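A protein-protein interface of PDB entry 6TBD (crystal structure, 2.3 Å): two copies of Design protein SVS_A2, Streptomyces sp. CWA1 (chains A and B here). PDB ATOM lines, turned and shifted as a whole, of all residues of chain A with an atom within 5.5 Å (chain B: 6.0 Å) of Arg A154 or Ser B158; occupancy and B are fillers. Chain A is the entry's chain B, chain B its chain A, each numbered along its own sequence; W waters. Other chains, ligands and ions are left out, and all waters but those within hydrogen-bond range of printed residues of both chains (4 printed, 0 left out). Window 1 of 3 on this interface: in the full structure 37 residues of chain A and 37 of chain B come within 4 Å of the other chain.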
ATOM      1  N   ASN A 104       6.493   2.415  23.054  1.00  0.00           N
ATOM      2  CA  ASN A 104       5.811   3.444  22.236  1.00  0.00           C
ATOM      3  C   ASN A 104       4.315   3.454  22.459  1.00  0.00           C
ATOM      4  O   ASN A 104       3.706   4.502  22.621  1.00  0.00           O
ATOM      5  CB  ASN A 104       6.138   3.264  20.783  1.00  0.00           C
ATOM      6  CG  ASN A 104       7.593   3.609  20.438  1.00  0.00           C
ATOM      7  OD1 ASN A 104       8.414   3.931  21.296  1.00  0.00           O
ATOM      8  ND2 ASN A 104       7.914   3.540  19.139  1.00  0.00           N
ATOM      9  N   GLN A 111       0.117   8.824  28.513  1.00  0.00           N
ATOM     10  CA  GLN A 111      -0.063  10.210  28.185  1.00  0.00           C
ATOM     11  C   GLN A 111      -1.527  10.557  27.888  1.00  0.00           C
ATOM     12  O   GLN A 111      -2.029  11.605  28.298  1.00  0.00           O
ATOM     13  CB  GLN A 111       0.844  10.544  26.988  1.00  0.00           C
ATOM     14  CG  GLN A 111       0.807  11.970  26.560  1.00  0.00           C
ATOM     15  CD  GLN A 111       1.394  12.877  27.565  1.00  0.00           C
ATOM     16  OE1 GLN A 111       2.260  12.477  28.361  1.00  0.00           O
ATOM     17  NE2 GLN A 111       0.979  14.119  27.526  1.00  0.00           N
ATOM     18  N   GLU A 115      -4.337  13.216  29.906  1.00  0.00           N
ATOM     19  CA  GLU A 115      -5.100  14.210  29.130  1.00  0.00           C
ATOM     20  C   GLU A 115      -6.604  13.994  29.118  1.00  0.00           C
ATOM     21  O   GLU A 115      -7.362  14.917  28.863  1.00  0.00           O
ATOM     22  CB  GLU A 115      -4.596  14.203  27.666  1.00  0.00           C
ATOM     23  CG  GLU A 115      -3.106  14.537  27.548  1.00  0.00           C
ATOM     24  CD  GLU A 115      -2.618  14.991  26.165  1.00  0.00           C
ATOM     25  OE1 GLU A 115      -1.469  14.650  25.797  1.00  0.00           O
ATOM     26  OE2 GLU A 115      -3.360  15.717  25.432  1.00  0.00           O
ATOM     27  N   ARG A 147      -1.966  22.001  30.805  1.00  0.00           N
ATOM     28  CA  ARG A 147      -1.430  21.703  29.476  1.00  0.00           C
ATOM     29  C   ARG A 147       0.057  21.739  29.396  1.00  0.00           C
ATOM     30  O   ARG A 147       0.675  20.908  28.734  1.00  0.00           O
ATOM     31  CB  ARG A 147      -1.993  22.604  28.380  1.00  0.00           C
ATOM     32  CG  ARG A 147      -3.389  22.312  27.951  1.00  0.00           C
ATOM     33  CD  ARG A 147      -3.565  20.879  27.567  1.00  0.00           C
ATOM     34  NE  ARG A 147      -3.133  20.553  26.225  1.00  0.00           N
ATOM     35  CZ  ARG A 147      -3.216  19.304  25.744  1.00  0.00           C
ATOM     36  NH1 ARG A 147      -3.672  18.302  26.526  1.00  0.00           N
ATOM     37  NH2 ARG A 147      -2.848  19.061  24.500  1.00  0.00           N
ATOM     38  N   PHE A 149       2.162  21.100  31.791  1.00  0.00           N
ATOM     39  CA  PHE A 149       2.661  19.898  32.415  1.00  0.00           C
ATOM     40  C   PHE A 149       2.442  18.735  31.423  1.00  0.00           C
ATOM     41  O   PHE A 149       3.324  17.917  31.235  1.00  0.00           O
ATOM     42  CB  PHE A 149       1.987  19.612  33.744  1.00  0.00           C
ATOM     43  CG  PHE A 149       2.426  18.335  34.334  1.00  0.00           C
ATOM     44  CD1 PHE A 149       3.595  18.268  35.058  1.00  0.00           C
ATOM     45  CD2 PHE A 149       1.753  17.173  34.057  1.00  0.00           C
ATOM     46  CE1 PHE A 149       4.061  17.068  35.596  1.00  0.00           C
ATOM     47  CE2 PHE A 149       2.206  15.976  34.551  1.00  0.00           C
ATOM     48  CZ  PHE A 149       3.354  15.911  35.350  1.00  0.00           C
ATOM     49  N   VAL A 150       1.286  18.695  30.770  1.00  0.00           N
ATOM     50  CA  VAL A 150       0.931  17.631  29.831  1.00  0.00           C
ATOM     51  C   VAL A 150       1.974  17.484  28.722  1.00  0.00           C
ATOM     52  O   VAL A 150       2.500  16.409  28.471  1.00  0.00           O
ATOM     53  CB  VAL A 150      -0.492  17.896  29.239  1.00  0.00           C
ATOM     54  CG1 VAL A 150      -0.720  17.149  27.964  1.00  0.00           C
ATOM     55  CG2 VAL A 150      -1.598  17.547  30.232  1.00  0.00           C
ATOM     56  N   HIS A 151       2.303  18.590  28.092  1.00  0.00           N
ATOM     57  CA  HIS A 151       3.276  18.605  27.006  1.00  0.00           C
ATOM     58  C   HIS A 151       4.704  18.280  27.487  1.00  0.00           C
ATOM     59  O   HIS A 151       5.446  17.608  26.801  1.00  0.00           O
ATOM     60  CB  HIS A 151       3.271  19.975  26.341  1.00  0.00           C
ATOM     61  CG  HIS A 151       2.014  20.303  25.611  1.00  0.00           C
ATOM     62  ND1 HIS A 151       1.350  19.384  24.827  1.00  0.00           N
ATOM     63  CD2 HIS A 151       1.329  21.467  25.483  1.00  0.00           C
ATOM     64  CE1 HIS A 151       0.274  19.945  24.299  1.00  0.00           C
ATOM     65  NE2 HIS A 151       0.255  21.208  24.659  1.00  0.00           N
ATOM     66  N   ALA A 152       5.087  18.751  28.681  1.00  0.00           N
ATOM     67  CA  ALA A 152       6.352  18.374  29.252  1.00  0.00           C
ATOM     68  C   ALA A 152       6.400  16.899  29.534  1.00  0.00           C
ATOM     69  O   ALA A 152       7.441  16.248  29.325  1.00  0.00           O
ATOM     70  CB  ALA A 152       6.644  19.150  30.534  1.00  0.00           C
ATOM     71  N   HIS A 153       5.286  16.373  29.997  1.00  0.00           N
ATOM     72  CA  HIS A 153       5.205  14.939  30.262  1.00  0.00           C
ATOM     73  C   HIS A 153       5.438  14.115  28.973  1.00  0.00           C
ATOM     74  O   HIS A 153       6.224  13.191  28.985  1.00  0.00           O
ATOM     75  CB  HIS A 153       3.893  14.635  30.880  1.00  0.00           C
ATOM     76  CG  HIS A 153       3.830  13.334  31.600  1.00  0.00           C
ATOM     77  ND1 HIS A 153       3.397  12.185  30.995  1.00  0.00           N
ATOM     78  CD2 HIS A 153       3.972  13.039  32.909  1.00  0.00           C
ATOM     79  CE1 HIS A 153       3.365  11.217  31.882  1.00  0.00           C
ATOM     80  NE2 HIS A 153       3.711  11.711  33.049  1.00  0.00           N
ATOM     81  N   ARG A 154       4.819  14.490  27.855  1.00  0.00           N
ATOM     82  CA  ARG A 154       5.021  13.800  26.605  1.00  0.00           C
ATOM     83  C   ARG A 154       6.486  13.873  26.174  1.00  0.00           C
ATOM     84  O   ARG A 154       7.051  12.871  25.700  1.00  0.00           O
ATOM     85  CB  ARG A 154       4.103  14.346  25.474  1.00  0.00           C
ATOM     86  CG  ARG A 154       4.257  13.559  24.174  1.00  0.00           C
ATOM     87  CD  ARG A 154       3.375  14.029  23.032  1.00  0.00           C
ATOM     88  NE  ARG A 154       2.024  13.465  23.171  1.00  0.00           N
ATOM     89  CZ  ARG A 154       0.913  14.126  23.465  1.00  0.00           C
ATOM     90  NH1 ARG A 154       0.886  15.462  23.558  1.00  0.00           N
ATOM     91  NH2 ARG A 154      -0.211  13.434  23.624  1.00  0.00           N
ATOM     92  N   ALA A 155       7.109  15.048  26.345  1.00  0.00           N
ATOM     93  CA  ALA A 155       8.516  15.247  25.927  1.00  0.00           C
ATOM     94  C   ALA A 155       9.455  14.324  26.665  1.00  0.00           C
ATOM     95  O   ALA A 155      10.331  13.727  26.091  1.00  0.00           O
ATOM     96  CB  ALA A 155       8.932  16.697  26.098  1.00  0.00           C
ATOM     97  N   TRP A 156       9.216  14.174  27.940  1.00  0.00           N
ATOM     98  CA  TRP A 156       9.933  13.251  28.778  1.00  0.00           C
ATOM     99  C   TRP A 156       9.736  11.846  28.237  1.00  0.00           C
ATOM    100  O   TRP A 156      10.724  11.142  28.011  1.00  0.00           O
ATOM    101  CB  TRP A 156       9.471  13.371  30.187  1.00  0.00           C
ATOM    102  CG  TRP A 156       9.832  12.292  31.031  1.00  0.00           C
ATOM    103  CD1 TRP A 156      11.075  11.919  31.331  1.00  0.00           C
ATOM    104  CD2 TRP A 156       8.943  11.376  31.718  1.00  0.00           C
ATOM    105  NE1 TRP A 156      11.062  10.847  32.168  1.00  0.00           N
ATOM    106  CE2 TRP A 156       9.769  10.474  32.430  1.00  0.00           C
ATOM    107  CE3 TRP A 156       7.552  11.239  31.811  1.00  0.00           C
ATOM    108  CZ2 TRP A 156       9.253   9.449  33.240  1.00  0.00           C
ATOM    109  CZ3 TRP A 156       7.018  10.191  32.601  1.00  0.00           C
ATOM    110  CH2 TRP A 156       7.868   9.310  33.306  1.00  0.00           C
ATOM    111  N   LEU A 157       8.503  11.460  27.947  1.00  0.00           N
ATOM    112  CA  LEU A 157       8.256  10.164  27.399  1.00  0.00           C
ATOM    113  C   LEU A 157       8.975   9.941  26.092  1.00  0.00           C
ATOM    114  O   LEU A 157       9.570   8.867  25.869  1.00  0.00           O
ATOM    115  CB  LEU A 157       6.778   9.936  27.281  1.00  0.00           C
ATOM    116  CG  LEU A 157       6.062   9.810  28.616  1.00  0.00           C
ATOM    117  CD1 LEU A 157       4.557   9.745  28.439  1.00  0.00           C
ATOM    118  CD2 LEU A 157       6.522   8.541  29.323  1.00  0.00           C
ATOM    119  N   SER A 158       8.966  10.933  25.214  1.00  0.00           N
ATOM    120  CA  SER A 158       9.746  10.846  23.973  1.00  0.00           C
ATOM    121  C   SER A 158      11.230  10.558  24.225  1.00  0.00           C
ATOM    122  O   SER A 158      11.890   9.807  23.497  1.00  0.00           O
ATOM    123  CB  SER A 158       9.565  12.116  23.126  1.00  0.00           C
ATOM    124  OG  SER A 158       8.174  12.215  22.828  1.00  0.00           O
ATOM    125  N   GLY A 159      11.778  11.188  25.232  1.00  0.00           N
ATOM    126  CA  GLY A 159      13.189  11.000  25.556  1.00  0.00           C
ATOM    127  C   GLY A 159      13.470   9.608  26.050  1.00  0.00           C
ATOM    128  O   GLY A 159      14.432   8.985  25.583  1.00  0.00           O
ATOM    129  N   HIS B 151       4.571  21.458  20.176  1.00  0.00           N
ATOM    130  CA  HIS B 151       4.012  20.448  21.046  1.00  0.00           C
ATOM    131  C   HIS B 151       3.063  19.534  20.248  1.00  0.00           C
ATOM    132  O   HIS B 151       3.046  18.325  20.455  1.00  0.00           O
ATOM    133  CB  HIS B 151       3.262  21.102  22.217  1.00  0.00           C
ATOM    134  CG  HIS B 151       4.148  21.660  23.268  1.00  0.00           C
ATOM    135  ND1 HIS B 151       5.314  21.046  23.673  1.00  0.00           N
ATOM    136  CD2 HIS B 151       4.038  22.778  24.001  1.00  0.00           C
ATOM    137  CE1 HIS B 151       5.886  21.778  24.598  1.00  0.00           C
ATOM    138  NE2 HIS B 151       5.117  22.818  24.832  1.00  0.00           N
ATOM    139  N   HIS B 153       3.386  18.821  17.178  1.00  0.00           N
ATOM    140  CA  HIS B 153       4.274  18.075  16.302  1.00  0.00           C
ATOM    141  C   HIS B 153       4.849  16.886  17.029  1.00  0.00           C
ATOM    142  O   HIS B 153       4.870  15.794  16.470  1.00  0.00           O
ATOM    143  CB  HIS B 153       5.379  19.006  15.760  1.00  0.00           C
ATOM    144  CG  HIS B 153       6.091  18.507  14.539  1.00  0.00           C
ATOM    145  ND1 HIS B 153       7.233  17.745  14.615  1.00  0.00           N
ATOM    146  CD2 HIS B 153       5.904  18.762  13.226  1.00  0.00           C
ATOM    147  CE1 HIS B 153       7.709  17.527  13.402  1.00  0.00           C
ATOM    148  NE2 HIS B 153       6.930  18.145  12.537  1.00  0.00           N
ATOM    149  N   ARG B 154       5.288  17.069  18.285  1.00  0.00           N
ATOM    150  CA  ARG B 154       5.781  15.949  19.025  1.00  0.00           C
ATOM    151  C   ARG B 154       4.644  14.971  19.246  1.00  0.00           C
ATOM    152  O   ARG B 154       4.851  13.772  19.200  1.00  0.00           O
ATOM    153  CB  ARG B 154       6.449  16.322  20.365  1.00  0.00           C
ATOM    154  CG  ARG B 154       6.902  15.028  21.094  1.00  0.00           C
ATOM    155  CD  ARG B 154       7.969  15.117  22.169  1.00  0.00           C
ATOM    156  NE  ARG B 154       7.998  16.426  22.654  1.00  0.00           N
ATOM    157  CZ  ARG B 154       9.007  17.276  22.632  1.00  0.00           C
ATOM    158  NH1 ARG B 154      10.246  16.923  22.282  1.00  0.00           N
ATOM    159  NH2 ARG B 154       8.736  18.517  23.050  1.00  0.00           N
ATOM    160  N   ALA B 155       3.448  15.482  19.516  1.00  0.00           N
ATOM    161  CA  ALA B 155       2.267  14.651  19.705  1.00  0.00           C
ATOM    162  C   ALA B 155       2.048  13.706  18.504  1.00  0.00           C
ATOM    163  O   ALA B 155       1.881  12.492  18.684  1.00  0.00           O
ATOM    164  CB  ALA B 155       1.049  15.530  19.987  1.00  0.00           C
ATOM    165  N   TRP B 156       2.131  14.284  17.297  1.00  0.00           N
ATOM    166  CA  TRP B 156       1.989  13.537  16.051  1.00  0.00           C
ATOM    167  C   TRP B 156       3.068  12.461  15.928  1.00  0.00           C
ATOM    168  O   TRP B 156       2.786  11.290  15.617  1.00  0.00           O
ATOM    169  CB  TRP B 156       2.048  14.476  14.863  1.00  0.00           C
ATOM    170  CG  TRP B 156       2.350  13.790  13.533  1.00  0.00           C
ATOM    171  CD1 TRP B 156       1.628  12.832  12.930  1.00  0.00           C
ATOM    172  CD2 TRP B 156       3.451  14.068  12.663  1.00  0.00           C
ATOM    173  NE1 TRP B 156       2.207  12.466  11.766  1.00  0.00           N
ATOM    174  CE2 TRP B 156       3.319  13.234  11.560  1.00  0.00           C
ATOM    175  CE3 TRP B 156       4.526  14.991  12.703  1.00  0.00           C
ATOM    176  CZ2 TRP B 156       4.225  13.247  10.505  1.00  0.00           C
ATOM    177  CZ3 TRP B 156       5.420  14.986  11.689  1.00  0.00           C
ATOM    178  CH2 TRP B 156       5.273  14.102  10.604  1.00  0.00           C
ATOM    179  N   LEU B 157       4.310  12.848  16.160  1.00  0.00           N
ATOM    180  CA  LEU B 157       5.412  11.897  16.094  1.00  0.00           C
ATOM    181  C   LEU B 157       5.237  10.803  17.153  1.00  0.00           C
ATOM    182  O   LEU B 157       5.575   9.646  16.878  1.00  0.00           O
ATOM    183  CB  LEU B 157       6.737  12.591  16.267  1.00  0.00           C
ATOM    184  CG  LEU B 157       7.218  13.512  15.158  1.00  0.00           C
ATOM    185  CD1 LEU B 157       8.526  14.149  15.567  1.00  0.00           C
ATOM    186  CD2 LEU B 157       7.413  12.720  13.881  1.00  0.00           C
ATOM    187  N   SER B 158       4.684  11.136  18.323  1.00  0.00           N
ATOM    188  CA  SER B 158       4.425  10.103  19.352  1.00  0.00           C
ATOM    189  C   SER B 158       3.359   9.129  18.831  1.00  0.00           C
ATOM    190  O   SER B 158       3.352   7.969  19.167  1.00  0.00           O
ATOM    191  CB  SER B 158       3.983  10.699  20.704  1.00  0.00           C
ATOM    192  OG  SER B 158       5.041  11.439  21.293  1.00  0.00           O
ATOM    193  N   GLY B 159       2.430   9.607  18.032  1.00  0.00           N
ATOM    194  CA  GLY B 159       1.380   8.734  17.481  1.00  0.00           C
ATOM    195  C   GLY B 159       1.991   7.833  16.451  1.00  0.00           C
ATOM    196  O   GLY B 159       1.679   6.633  16.395  1.00  0.00           O
ATOM    197  N   VAL B 160       2.859   8.403  15.616  1.00  0.00           N
ATOM    198  CA  VAL B 160       3.522   7.608  14.570  1.00  0.00           C
ATOM    199  C   VAL B 160       4.402   6.555  15.204  1.00  0.00           C
ATOM    200  O   VAL B 160       4.382   5.427  14.762  1.00  0.00           O
ATOM    201  CB  VAL B 160       4.318   8.483  13.603  1.00  0.00           C
ATOM    202  CG1 VAL B 160       5.041   7.619  12.573  1.00  0.00           C
ATOM    203  CG2 VAL B 160       3.373   9.440  12.860  1.00  0.00           C
ATOM    204  N   ALA B 161       5.160   6.919  16.238  1.00  0.00           N
ATOM    205  CA  ALA B 161       6.010   5.958  16.949  1.00  0.00           C
ATOM    206  C   ALA B 161       5.187   4.823  17.485  1.00  0.00           C
ATOM    207  O   ALA B 161       5.573   3.698  17.369  1.00  0.00           O
ATOM    208  CB  ALA B 161       6.784   6.621  18.113  1.00  0.00           C
ATOM    209  N   TRP B 162       4.048   5.154  18.099  1.00  0.00           N
ATOM    210  CA  TRP B 162       3.098   4.187  18.621  1.00  0.00           C
ATOM    211  C   TRP B 162       2.640   3.281  17.466  1.00  0.00           C
ATOM    212  O   TRP B 162       2.645   2.075  17.568  1.00  0.00           O
ATOM    213  CB  TRP B 162       1.930   4.955  19.258  1.00  0.00           C
ATOM    214  CG  TRP B 162       0.794   4.195  19.914  1.00  0.00           C
ATOM    215  CD1 TRP B 162       0.548   2.850  19.897  1.00  0.00           C
ATOM    216  CD2 TRP B 162      -0.291   4.788  20.653  1.00  0.00           C
ATOM    217  NE1 TRP B 162      -0.589   2.567  20.617  1.00  0.00           N
ATOM    218  CE2 TRP B 162      -1.121   3.737  21.091  1.00  0.00           C
ATOM    219  CE3 TRP B 162      -0.603   6.111  21.028  1.00  0.00           C
ATOM    220  CZ2 TRP B 162      -2.261   3.955  21.890  1.00  0.00           C
ATOM    221  CZ3 TRP B 162      -1.727   6.331  21.809  1.00  0.00           C
ATOM    222  CH2 TRP B 162      -2.561   5.256  22.231  1.00  0.00           C
ATOM    223  N   GLN B 163       2.257   3.883  16.362  1.00  0.00           N
ATOM    224  CA  GLN B 163       1.807   3.134  15.219  1.00  0.00           C
ATOM    225  C   GLN B 163       2.915   2.201  14.616  1.00  0.00           C
ATOM    226  O   GLN B 163       2.629   1.053  14.266  1.00  0.00           O
ATOM    227  CB  GLN B 163       1.292   4.105  14.189  1.00  0.00           C
ATOM    228  CG  GLN B 163       0.651   3.507  12.962  1.00  0.00           C
ATOM    229  CD  GLN B 163       0.542   4.570  11.880  1.00  0.00           C
ATOM    230  OE1 GLN B 163      -0.203   5.561  12.048  1.00  0.00           O
ATOM    231  NE2 GLN B 163       1.327   4.429  10.802  1.00  0.00           N
ATOM    232  N   LEU B 184      -3.431  11.207  17.086  1.00  0.00           N
ATOM    233  CA  LEU B 184      -2.095  11.719  16.923  1.00  0.00           C
ATOM    234  C   LEU B 184      -1.426  11.409  15.555  1.00  0.00           C
ATOM    235  O   LEU B 184      -0.842  12.268  14.930  1.00  0.00           O
ATOM    236  CB  LEU B 184      -1.258  11.184  18.089  1.00  0.00           C
ATOM    237  CG  LEU B 184      -1.753  11.531  19.498  1.00  0.00           C
ATOM    238  CD1 LEU B 184      -0.716  11.135  20.568  1.00  0.00           C
ATOM    239  CD2 LEU B 184      -2.144  13.011  19.694  1.00  0.00           C
HETATM  240  O   HOH W   1       7.558  12.251  20.161  1.00  0.00           O
HETATM  241  O   HOH W   2       5.698  17.865  24.087  1.00  0.00           O
HETATM  242  O   HOH W   3       3.116  17.393  23.055  1.00  0.00           O
HETATM  243  O   HOH W   4       5.994  10.473  23.563  1.00  0.00           O
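O of Ala B161 sits at hydrogen-bond distance from ND2 of Asn A104, 2.9 Å away.
The side-chain amide oxygen of Gln A111 is in hydrogen-bond range of the backbone NH of Arg A154 (3.3 Å). The guanidinium group of Arg A154 lies within salt-bridge range of the side-chain carboxylate of Glu A115 (2.8 Å). The backbone carbonyl oxygen (O) of Arg B154 is in hydrogen-bond range of the side-chain hydroxyl (OG) of Ser B158. OG of Ser A158 sits at hydrogen-bond distance from O of Arg A154, at 3.2 Å.
Asn A104 touches Trp B162 (O to CB, 3.8 Å). CD2 of His A151 touches CD2 of His B151, 3.4 Å away. Arg A154 touches Ala B155. Arg A154 touches Ser B158. Leu B184 touches Arg A154. Arg B154 touches Ala A155. Arg B154 touches Ser A158 (CD to OG, 3.0 Å). Ser A158 touches Ser B158 (OG to OG, 3.6 Å).
Of the printed residues of chain B, Arg A154 touches Ala B155, Ser B158 and Leu B184. Ser B158 touches two residues of chain A. Of the printed residues of chain A, His B151 touches His A151. Printed residues of chain A within 4 Å of Leu B184: Arg A154 (3.9 Å). Printed residues of chain B within 4 Å of Ala A155: Arg B154. Of the printed residues of chain A, Arg B154 touches Ala A155 and Ser A158. Leu B157 touches none of the printed residues of chain A. The nearest residue of chain B that does not touch Arg A154 is Arg B154 (4.1 Å). The nearest residue of chain A that does not touch Ser B158 is Asn A104 (4.9 Å). The nearest printed residue of chain A that does not touch Ala B161 is Ser A158 (7.4 Å).
Of the 13 printed residues of chain B, 7 touch a printed residue of chain A. Printed residues of chain B that touch a printed residue of chain A: His B151, Arg B154, Ala B155, Ser B158, Ala B161, Trp B162 and Leu B184. Hydrophobic or aromatic side chains of chain B that line the printed part of chain A: His B151, Ala B155, Ala B161, Trp B162 and Leu B184. Of the 15 printed residues of chain A, 5 touch a printed residue of chain B. Among the printed residues, 9 pairs touch across the chains.
His B151 touches its own counterpart, His A151. Arg A154 touches Ala B155, and with the chains exchanged Ala A155 touches Arg B154. Arg A154 touches Ser B158, and with the chains exchanged Ser A158 touches Arg B154. Ser A158 touches its own counterpart, Ser B158.
Water W4 lies within hydrogen-bond range of OG of Ser B158 (2.6 Å), OG of Ser A158 (2.9 Å) and O of Arg A154 (3.4 Å). Water W1 lies within hydrogen-bond range of OG of Ser A158 (2.7 Å), OG of Ser B158 (2.9 Å) and O of Arg B154 (3.3 Å). Water W2 lies within hydrogen-bond range of O of His A151 (2.7 Å), NE of Arg B154 (3.1 Å) and ND1 of His B151 (3.2 Å). Water W3 lies within hydrogen-bond range of O of His B151, NH1 of Arg A154 and ND1 of His A151.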
